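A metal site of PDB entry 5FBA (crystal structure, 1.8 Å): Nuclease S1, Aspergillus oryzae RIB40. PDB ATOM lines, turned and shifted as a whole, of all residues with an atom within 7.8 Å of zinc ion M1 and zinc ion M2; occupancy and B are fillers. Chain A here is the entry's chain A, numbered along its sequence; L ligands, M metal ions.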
ATOM      1  N   TRP A   1      -5.427  -6.768   9.637  1.00  0.00           N
ATOM      2  CA  TRP A   1      -4.375  -6.093   8.840  1.00  0.00           C
ATOM      3  C   TRP A   1      -3.464  -7.181   8.287  1.00  0.00           C
ATOM      4  O   TRP A   1      -3.391  -8.319   8.812  1.00  0.00           O
ATOM      5  CB  TRP A   1      -3.525  -5.117   9.671  1.00  0.00           C
ATOM      6  CG  TRP A   1      -4.274  -4.064  10.440  1.00  0.00           C
ATOM      7  CD1 TRP A   1      -4.547  -4.075  11.772  1.00  0.00           C
ATOM      8  CD2 TRP A   1      -4.880  -2.851   9.906  1.00  0.00           C
ATOM      9  NE1 TRP A   1      -5.234  -2.928  12.126  1.00  0.00           N
ATOM     10  CE2 TRP A   1      -5.495  -2.184  11.002  1.00  0.00           C
ATOM     11  CE3 TRP A   1      -4.978  -2.294   8.628  1.00  0.00           C
ATOM     12  CZ2 TRP A   1      -6.176  -0.989  10.867  1.00  0.00           C
ATOM     13  CZ3 TRP A   1      -5.685  -1.059   8.478  1.00  0.00           C
ATOM     14  CH2 TRP A   1      -6.278  -0.422   9.611  1.00  0.00           C
ATOM     15  N   GLY A   2      -2.754  -6.817   7.246  1.00  0.00           N
ATOM     16  CA  GLY A   2      -1.623  -7.645   6.761  1.00  0.00           C
ATOM     17  C   GLY A   2      -0.425  -7.386   7.643  1.00  0.00           C
ATOM     18  O   GLY A   2      -0.549  -6.707   8.671  1.00  0.00           O
ATOM     19  N   ASN A   3       0.733  -7.898   7.238  1.00  0.00           N
ATOM     20  CA  ASN A   3       1.922  -7.916   8.092  1.00  0.00           C
ATOM     21  C   ASN A   3       2.391  -6.529   8.456  1.00  0.00           C
ATOM     22  O   ASN A   3       2.722  -6.271   9.581  1.00  0.00           O
ATOM     23  CB  ASN A   3       3.047  -8.698   7.413  1.00  0.00           C
ATOM     24  CG  ASN A   3       2.680 -10.174   7.251  1.00  0.00           C
ATOM     25  OD1 ASN A   3       1.754 -10.713   7.879  1.00  0.00           O
ATOM     26  ND2 ASN A   3       3.369 -10.815   6.374  1.00  0.00           N
ATOM     27  N   GLY A   5       0.727  -3.596   8.644  1.00  0.00           N
ATOM     28  CA  GLY A   5      -0.189  -3.099   9.657  1.00  0.00           C
ATOM     29  C   GLY A   5       0.110  -3.635  11.069  1.00  0.00           C
ATOM     30  O   GLY A   5       0.222  -2.877  11.999  1.00  0.00           O
ATOM     31  N   HIS A   6       0.203  -4.942  11.207  1.00  0.00           N
ATOM     32  CA  HIS A   6       0.512  -5.545  12.515  1.00  0.00           C
ATOM     33  C   HIS A   6       1.838  -5.158  13.094  1.00  0.00           C
ATOM     34  O   HIS A   6       1.950  -4.916  14.310  1.00  0.00           O
ATOM     35  CB  HIS A   6       0.401  -7.031  12.400  1.00  0.00           C
ATOM     36  CG  HIS A   6      -1.006  -7.476  12.395  1.00  0.00           C
ATOM     37  ND1 HIS A   6      -1.862  -7.220  13.441  1.00  0.00           N
ATOM     38  CD2 HIS A   6      -1.746  -8.064  11.436  1.00  0.00           C
ATOM     39  CE1 HIS A   6      -3.049  -7.720  13.165  1.00  0.00           C
ATOM     40  NE2 HIS A   6      -3.021  -8.224  11.948  1.00  0.00           N
ATOM     41  N   ALA A  41       4.263 -10.040  15.833  1.00  0.00           N
ATOM     42  CA  ALA A  41       2.993  -9.405  15.580  1.00  0.00           C
ATOM     43  C   ALA A  41       2.181 -10.095  14.459  1.00  0.00           C
ATOM     44  O   ALA A  41       0.976  -9.838  14.376  1.00  0.00           O
ATOM     45  CB  ALA A  41       3.197  -7.911  15.271  1.00  0.00           C
ATOM     46  N   THR A  42       2.817 -10.901  13.610  1.00  0.00           N
ATOM     47  CA  THR A  42       2.105 -11.582  12.484  1.00  0.00           C
ATOM     48  C   THR A  42       1.905 -13.058  12.743  1.00  0.00           C
ATOM     49  O   THR A  42       1.273 -13.750  11.934  1.00  0.00           O
ATOM     50  CB  THR A  42       2.849 -11.429  11.149  1.00  0.00           C
ATOM     51  OG1 THR A  42       4.065 -12.155  11.269  1.00  0.00           O
ATOM     52  CG2 THR A  42       3.226  -9.983  10.903  1.00  0.00           C
ATOM     53  N   ALA A  44       0.074 -14.868  14.625  1.00  0.00           N
ATOM     54  CA  ALA A  44      -1.267 -15.439  14.638  1.00  0.00           C
ATOM     55  C   ALA A  44      -1.833 -15.685  13.220  1.00  0.00           C
ATOM     56  O   ALA A  44      -2.616 -16.636  13.030  1.00  0.00           O
ATOM     57  CB  ALA A  44      -2.205 -14.609  15.500  1.00  0.00           C
ATOM     58  N   ASP A  45      -1.398 -14.905  12.253  1.00  0.00           N
ATOM     59  CA  ASP A  45      -1.804 -15.031  10.862  1.00  0.00           C
ATOM     60  C   ASP A  45      -1.148 -16.268  10.168  1.00  0.00           C
ATOM     61  O   ASP A  45      -1.792 -16.891   9.351  1.00  0.00           O
ATOM     62  CB  ASP A  45      -1.548 -13.752  10.034  1.00  0.00           C
ATOM     63  CG  ASP A  45      -2.695 -12.725  10.164  1.00  0.00           C
ATOM     64  OD1 ASP A  45      -3.784 -13.036  10.746  1.00  0.00           O
ATOM     65  OD2 ASP A  45      -2.488 -11.572   9.672  1.00  0.00           O
ATOM     66  N   THR A  46       0.033 -16.656  10.603  1.00  0.00           N
ATOM     67  CA  THR A  46       0.592 -17.982  10.297  1.00  0.00           C
ATOM     68  C   THR A  46      -0.146 -19.139  10.949  1.00  0.00           C
ATOM     69  O   THR A  46      -0.520 -20.123  10.319  1.00  0.00           O
ATOM     70  CB  THR A  46       2.081 -17.966  10.685  1.00  0.00           C
ATOM     71  OG1 THR A  46       2.750 -17.156   9.737  1.00  0.00           O
ATOM     72  CG2 THR A  46       2.710 -19.362  10.706  1.00  0.00           C
ATOM     73  N   LYS A  48      -3.060 -19.565  12.221  1.00  0.00           N
ATOM     74  CA  LYS A  48      -4.407 -19.910  11.793  1.00  0.00           C
ATOM     75  C   LYS A  48      -4.481 -20.756  10.507  1.00  0.00           C
ATOM     76  O   LYS A  48      -5.519 -21.332  10.240  1.00  0.00           O
ATOM     77  CB  LYS A  48      -5.258 -18.617  11.658  1.00  0.00           C
ATOM     78  CG  LYS A  48      -5.017 -17.870  10.380  1.00  0.00           C
ATOM     79  CD  LYS A  48      -5.676 -16.529  10.414  1.00  0.00           C
ATOM     80  CE  LYS A  48      -5.486 -15.748   9.135  1.00  0.00           C
ATOM     81  NZ  LYS A  48      -5.932 -14.365   9.368  1.00  0.00           N
ATOM     82  N   SER A  56      -8.173 -21.119  15.787  1.00  0.00           N
ATOM     83  CA  SER A  56      -7.968 -19.709  16.027  1.00  0.00           C
ATOM     84  C   SER A  56      -8.363 -18.755  14.890  1.00  0.00           C
ATOM     85  O   SER A  56      -8.266 -17.561  15.094  1.00  0.00           O
ATOM     86  CB  SER A  56      -6.480 -19.462  16.424  1.00  0.00           C
ATOM     87  OG  SER A  56      -5.565 -19.773  15.373  1.00  0.00           O
ATOM     88  N   LYS A  57      -8.789 -19.240  13.717  1.00  0.00           N
ATOM     89  CA  LYS A  57      -9.182 -18.340  12.616  1.00  0.00           C
ATOM     90  C   LYS A  57     -10.261 -17.271  13.016  1.00  0.00           C
ATOM     91  O   LYS A  57     -10.122 -16.119  12.680  1.00  0.00           O
ATOM     92  CB  LYS A  57      -9.746 -19.112  11.425  1.00  0.00           C
ATOM     93  CG  LYS A  57      -8.721 -19.782  10.523  1.00  0.00           C
ATOM     94  CD  LYS A  57      -9.475 -20.435   9.378  1.00  0.00           C
ATOM     95  CE  LYS A  57      -8.744 -21.655   8.805  1.00  0.00           C
ATOM     96  NZ  LYS A  57      -7.929 -21.301   7.605  1.00  0.00           N
ATOM     97  N   TYR A  59     -10.743 -15.900  15.800  1.00  0.00           N
ATOM     98  CA  TYR A  59     -10.205 -14.955  16.795  1.00  0.00           C
ATOM     99  C   TYR A  59      -9.726 -13.664  16.205  1.00  0.00           C
ATOM    100  O   TYR A  59      -9.394 -12.725  16.939  1.00  0.00           O
ATOM    101  CB  TYR A  59      -9.116 -15.567  17.683  1.00  0.00           C
ATOM    102  CG  TYR A  59      -9.464 -16.882  18.442  1.00  0.00           C
ATOM    103  CD1 TYR A  59     -10.750 -17.433  18.444  1.00  0.00           C
ATOM    104  CD2 TYR A  59      -8.480 -17.523  19.205  1.00  0.00           C
ATOM    105  CE1 TYR A  59     -11.022 -18.617  19.144  1.00  0.00           C
ATOM    106  CE2 TYR A  59      -8.756 -18.644  19.928  1.00  0.00           C
ATOM    107  CZ  TYR A  59     -10.029 -19.193  19.889  1.00  0.00           C
ATOM    108  OH  TYR A  59     -10.259 -20.363  20.552  1.00  0.00           O
ATOM    109  N   HIS A  60      -9.727 -13.552  14.860  1.00  0.00           N
ATOM    110  CA  HIS A  60      -9.253 -12.341  14.235  1.00  0.00           C
ATOM    111  C   HIS A  60     -10.318 -11.284  14.036  1.00  0.00           C
ATOM    112  O   HIS A  60      -9.964 -10.164  13.651  1.00  0.00           O
ATOM    113  CB  HIS A  60      -8.575 -12.693  12.903  1.00  0.00           C
ATOM    114  CG  HIS A  60      -7.372 -13.560  13.111  1.00  0.00           C
ATOM    115  ND1 HIS A  60      -6.095 -13.123  12.834  1.00  0.00           N
ATOM    116  CD2 HIS A  60      -7.244 -14.752  13.749  1.00  0.00           C
ATOM    117  CE1 HIS A  60      -5.232 -14.047  13.233  1.00  0.00           C
ATOM    118  NE2 HIS A  60      -5.912 -15.044  13.775  1.00  0.00           N
ATOM    119  N   PHE A  61     -11.578 -11.656  14.269  1.00  0.00           N
ATOM    120  CA  PHE A  61     -12.657 -10.753  13.969  1.00  0.00           C
ATOM    121  C   PHE A  61     -13.862 -10.922  14.891  1.00  0.00           C
ATOM    122  O   PHE A  61     -13.968 -11.865  15.670  1.00  0.00           O
ATOM    123  CB  PHE A  61     -13.073 -10.895  12.493  1.00  0.00           C
ATOM    124  CG  PHE A  61     -13.402 -12.299  12.070  1.00  0.00           C
ATOM    125  CD1 PHE A  61     -14.664 -12.819  12.230  1.00  0.00           C
ATOM    126  CD2 PHE A  61     -12.420 -13.100  11.500  1.00  0.00           C
ATOM    127  CE1 PHE A  61     -14.960 -14.101  11.853  1.00  0.00           C
ATOM    128  CE2 PHE A  61     -12.702 -14.411  11.111  1.00  0.00           C
ATOM    129  CZ  PHE A  61     -13.985 -14.909  11.280  1.00  0.00           C
ATOM    130  N   HIS A 115      -1.347  -9.275  18.273  1.00  0.00           N
ATOM    131  CA  HIS A 115      -1.936  -9.380  16.942  1.00  0.00           C
ATOM    132  C   HIS A 115      -3.396  -8.880  16.963  1.00  0.00           C
ATOM    133  O   HIS A 115      -3.798  -8.017  16.192  1.00  0.00           O
ATOM    134  CB  HIS A 115      -1.881 -10.820  16.413  1.00  0.00           C
ATOM    135  CG  HIS A 115      -2.381 -10.944  15.022  1.00  0.00           C
ATOM    136  ND1 HIS A 115      -1.571 -10.697  13.920  1.00  0.00           N
ATOM    137  CD2 HIS A 115      -3.598 -11.271  14.526  1.00  0.00           C
ATOM    138  CE1 HIS A 115      -2.277 -10.841  12.817  1.00  0.00           C
ATOM    139  NE2 HIS A 115      -3.511 -11.174  13.150  1.00  0.00           N
ATOM    140  N   ILE A 116      -4.153  -9.399  17.923  1.00  0.00           N
ATOM    141  CA  ILE A 116      -5.635  -9.211  17.917  1.00  0.00           C
ATOM    142  C   ILE A 116      -6.050  -7.807  18.273  1.00  0.00           C
ATOM    143  O   ILE A 116      -6.947  -7.282  17.632  1.00  0.00           O
ATOM    144  CB  ILE A 116      -6.350 -10.257  18.737  1.00  0.00           C
ATOM    145  CG1 ILE A 116      -6.176 -11.601  18.036  1.00  0.00           C
ATOM    146  CG2 ILE A 116      -7.856  -9.974  18.847  1.00  0.00           C
ATOM    147  CD1 ILE A 116      -6.439 -12.808  18.946  1.00  0.00           C
ATOM    148  N   GLY A 118      -4.428  -5.364  17.314  1.00  0.00           N
ATOM    149  CA  GLY A 118      -4.321  -4.854  15.901  1.00  0.00           C
ATOM    150  C   GLY A 118      -5.571  -5.064  15.055  1.00  0.00           C
ATOM    151  O   GLY A 118      -6.162  -4.099  14.547  1.00  0.00           O
ATOM    152  N   ASP A 119      -5.962  -6.321  14.924  1.00  0.00           N
ATOM    153  CA  ASP A 119      -7.142  -6.686  14.148  1.00  0.00           C
ATOM    154  C   ASP A 119      -8.472  -5.960  14.526  1.00  0.00           C
ATOM    155  O   ASP A 119      -9.267  -5.576  13.652  1.00  0.00           O
ATOM    156  CB  ASP A 119      -7.343  -8.191  14.218  1.00  0.00           C
ATOM    157  CG  ASP A 119      -6.533  -8.928  13.176  1.00  0.00           C
ATOM    158  OD1 ASP A 119      -6.026  -8.217  12.268  1.00  0.00           O
ATOM    159  OD2 ASP A 119      -6.475 -10.182  13.222  1.00  0.00           O
ATOM    160  N   ILE A 120      -8.661  -5.770  15.812  1.00  0.00           N
ATOM    161  CA  ILE A 120      -9.855  -5.119  16.344  1.00  0.00           C
ATOM    162  C   ILE A 120      -9.983  -3.710  15.782  1.00  0.00           C
ATOM    163  O   ILE A 120     -11.090  -3.188  15.659  1.00  0.00           O
ATOM    164  CB  ILE A 120      -9.831  -5.165  17.885  1.00  0.00           C
ATOM    165  CG1 ILE A 120     -10.207  -6.566  18.357  1.00  0.00           C
ATOM    166  CG2 ILE A 120     -10.796  -4.144  18.477  1.00  0.00           C
ATOM    167  CD1 ILE A 120      -9.887  -6.803  19.824  1.00  0.00           C
ATOM    168  N   GLN A 122      -8.996  -2.825  12.684  1.00  0.00           N
ATOM    169  CA  GLN A 122      -9.213  -2.833  11.211  1.00  0.00           C
ATOM    170  C   GLN A 122     -10.747  -2.893  11.119  1.00  0.00           C
ATOM    171  O   GLN A 122     -11.318  -3.916  11.488  1.00  0.00           O
ATOM    172  CB  GLN A 122      -8.525  -4.053  10.572  1.00  0.00           C
ATOM    173  CG  GLN A 122      -8.153  -3.926   9.113  1.00  0.00           C
ATOM    174  CD  GLN A 122      -9.365  -3.941   8.175  1.00  0.00           C
ATOM    175  OE1 GLN A 122     -10.273  -3.131   8.301  1.00  0.00           O
ATOM    176  NE2 GLN A 122      -9.366  -4.852   7.232  1.00  0.00           N
ATOM    177  N   HIS A 125     -12.527  -6.058  10.166  1.00  0.00           N
ATOM    178  CA  HIS A 125     -12.489  -7.151  11.091  1.00  0.00           C
ATOM    179  C   HIS A 125     -13.615  -7.021  12.170  1.00  0.00           C
ATOM    180  O   HIS A 125     -13.696  -7.857  13.087  1.00  0.00           O
ATOM    181  CB  HIS A 125     -11.122  -7.192  11.720  1.00  0.00           C
ATOM    182  CG  HIS A 125     -10.080  -7.857  10.869  1.00  0.00           C
ATOM    183  ND1 HIS A 125      -9.461  -9.009  11.268  1.00  0.00           N
ATOM    184  CD2 HIS A 125      -9.583  -7.548   9.658  1.00  0.00           C
ATOM    185  CE1 HIS A 125      -8.598  -9.377  10.339  1.00  0.00           C
ATOM    186  NE2 HIS A 125      -8.663  -8.509   9.352  1.00  0.00           N
ATOM    187  N   HIS A 148     -11.798  -6.110   1.598  1.00  0.00           N
ATOM    188  CA  HIS A 148     -11.064  -6.453   2.810  1.00  0.00           C
ATOM    189  C   HIS A 148      -9.532  -6.375   2.648  1.00  0.00           C
ATOM    190  O   HIS A 148      -8.827  -5.814   3.506  1.00  0.00           O
ATOM    191  CB  HIS A 148     -11.456  -7.831   3.277  1.00  0.00           C
ATOM    192  CG  HIS A 148     -10.893  -8.149   4.613  1.00  0.00           C
ATOM    193  ND1 HIS A 148     -11.660  -8.182   5.752  1.00  0.00           N
ATOM    194  CD2 HIS A 148      -9.622  -8.417   4.978  1.00  0.00           C
ATOM    195  CE1 HIS A 148     -10.875  -8.484   6.767  1.00  0.00           C
ATOM    196  NE2 HIS A 148      -9.632  -8.569   6.332  1.00  0.00           N
ATOM    197  N   ASP A 152      -6.698  -4.320   4.720  1.00  0.00           N
ATOM    198  CA  ASP A 152      -5.619  -5.058   5.324  1.00  0.00           C
ATOM    199  C   ASP A 152      -4.223  -4.647   4.883  1.00  0.00           C
ATOM    200  O   ASP A 152      -3.325  -4.524   5.721  1.00  0.00           O
ATOM    201  CB  ASP A 152      -5.757  -6.565   5.109  1.00  0.00           C
ATOM    202  CG  ASP A 152      -6.566  -7.234   6.210  1.00  0.00           C
ATOM    203  OD1 ASP A 152      -6.989  -6.586   7.183  1.00  0.00           O
ATOM    204  OD2 ASP A 152      -6.812  -8.427   6.017  1.00  0.00           O
ATOM    205  N   THR A 153      -4.069  -4.445   3.571  1.00  0.00           N
ATOM    206  CA  THR A 153      -2.769  -4.523   2.924  1.00  0.00           C
ATOM    207  C   THR A 153      -2.462  -3.462   1.881  1.00  0.00           C
ATOM    208  O   THR A 153      -1.528  -2.685   2.070  1.00  0.00           O
ATOM    209  CB  THR A 153      -2.640  -5.918   2.311  1.00  0.00           C
ATOM    210  OG1 THR A 153      -2.606  -6.836   3.382  1.00  0.00           O
ATOM    211  CG2 THR A 153      -1.321  -6.094   1.458  1.00  0.00           C
HETATM  212  P1  LIG L   1      -5.685 -10.856   9.195  1.00  0.00           P
HETATM  213  O1  LIG L   1      -5.079 -10.374  10.501  1.00  0.00           O
HETATM  214  O2  LIG L   1      -4.613 -11.420   8.298  1.00  0.00           O
HETATM  215  O3  LIG L   1      -6.310  -9.673   8.490  1.00  0.00           O
HETATM  216  O4  LIG L   1      -6.679 -11.949   9.497  1.00  0.00           O
HETATM  217 ZN    ZN M   1      -4.654  -8.463  10.647  1.00  0.00          ZN
HETATM  218 ZN    ZN M   2      -5.283 -11.393  12.050  1.00  0.00          ZN
HETATM  219 ZN    ZN M   3      -7.970  -9.060   7.496  1.00  0.00          ZN
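O1 of the ligand binds zinc ion M1 (2.0 Å). Zinc ion M1 is bound by a ring nitrogen (NE2) of His 6, at 2.1 Å. Zinc ion M1 is bound by the backbone nitrogen (N) of Trp 1 (2.1 Å). OD1 of Asp 119 is bound to zinc ion M1, at 2.1 Å. Zinc ion M1 is bound by O of Trp 1 (2.2 Å).
OD1 of Asp 45 lies close to NZ of Lys 48. The backbone NH (N) of Trp 1 lies close to the side-chain carboxylate (OD1) of Asp 152, 2.9 Å away. The backbone carbonyl oxygen of His 115 sits close to a ring nitrogen (ND1) of His 6, 3.5 Å away. The backbone carbonyl oxygen of Gly 118 is in hydrogen-bond range of the indole nitrogen of Trp 1, at 2.8 Å. O of Ala 41 is in hydrogen-bond range of ND1 of His 115. O of His 60 sits at hydrogen-bond distance from ND1 of His 125.
The nearest printed residue that does not touch zinc ion M2 is Lys 48 (4.1 Å).
Zinc ion M2 is bound by an oxygen (O1) of the ligand (1.9 Å), the side-chain carboxylate of Asp 119 (2.1 Å), a ring nitrogen (ND1) of His 60 (2.1 Å), a ring nitrogen (NE2) of His 115 (2.1 Å) and the side-chain carboxylate of Asp 45 (2.6 Å). Zinc ion M2 has five donor atoms within binding distance.
Five residues have an atom within 4 Å of zinc ion M1: Trp 1, His 6, Asp 45, His 115 and Asp 119.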
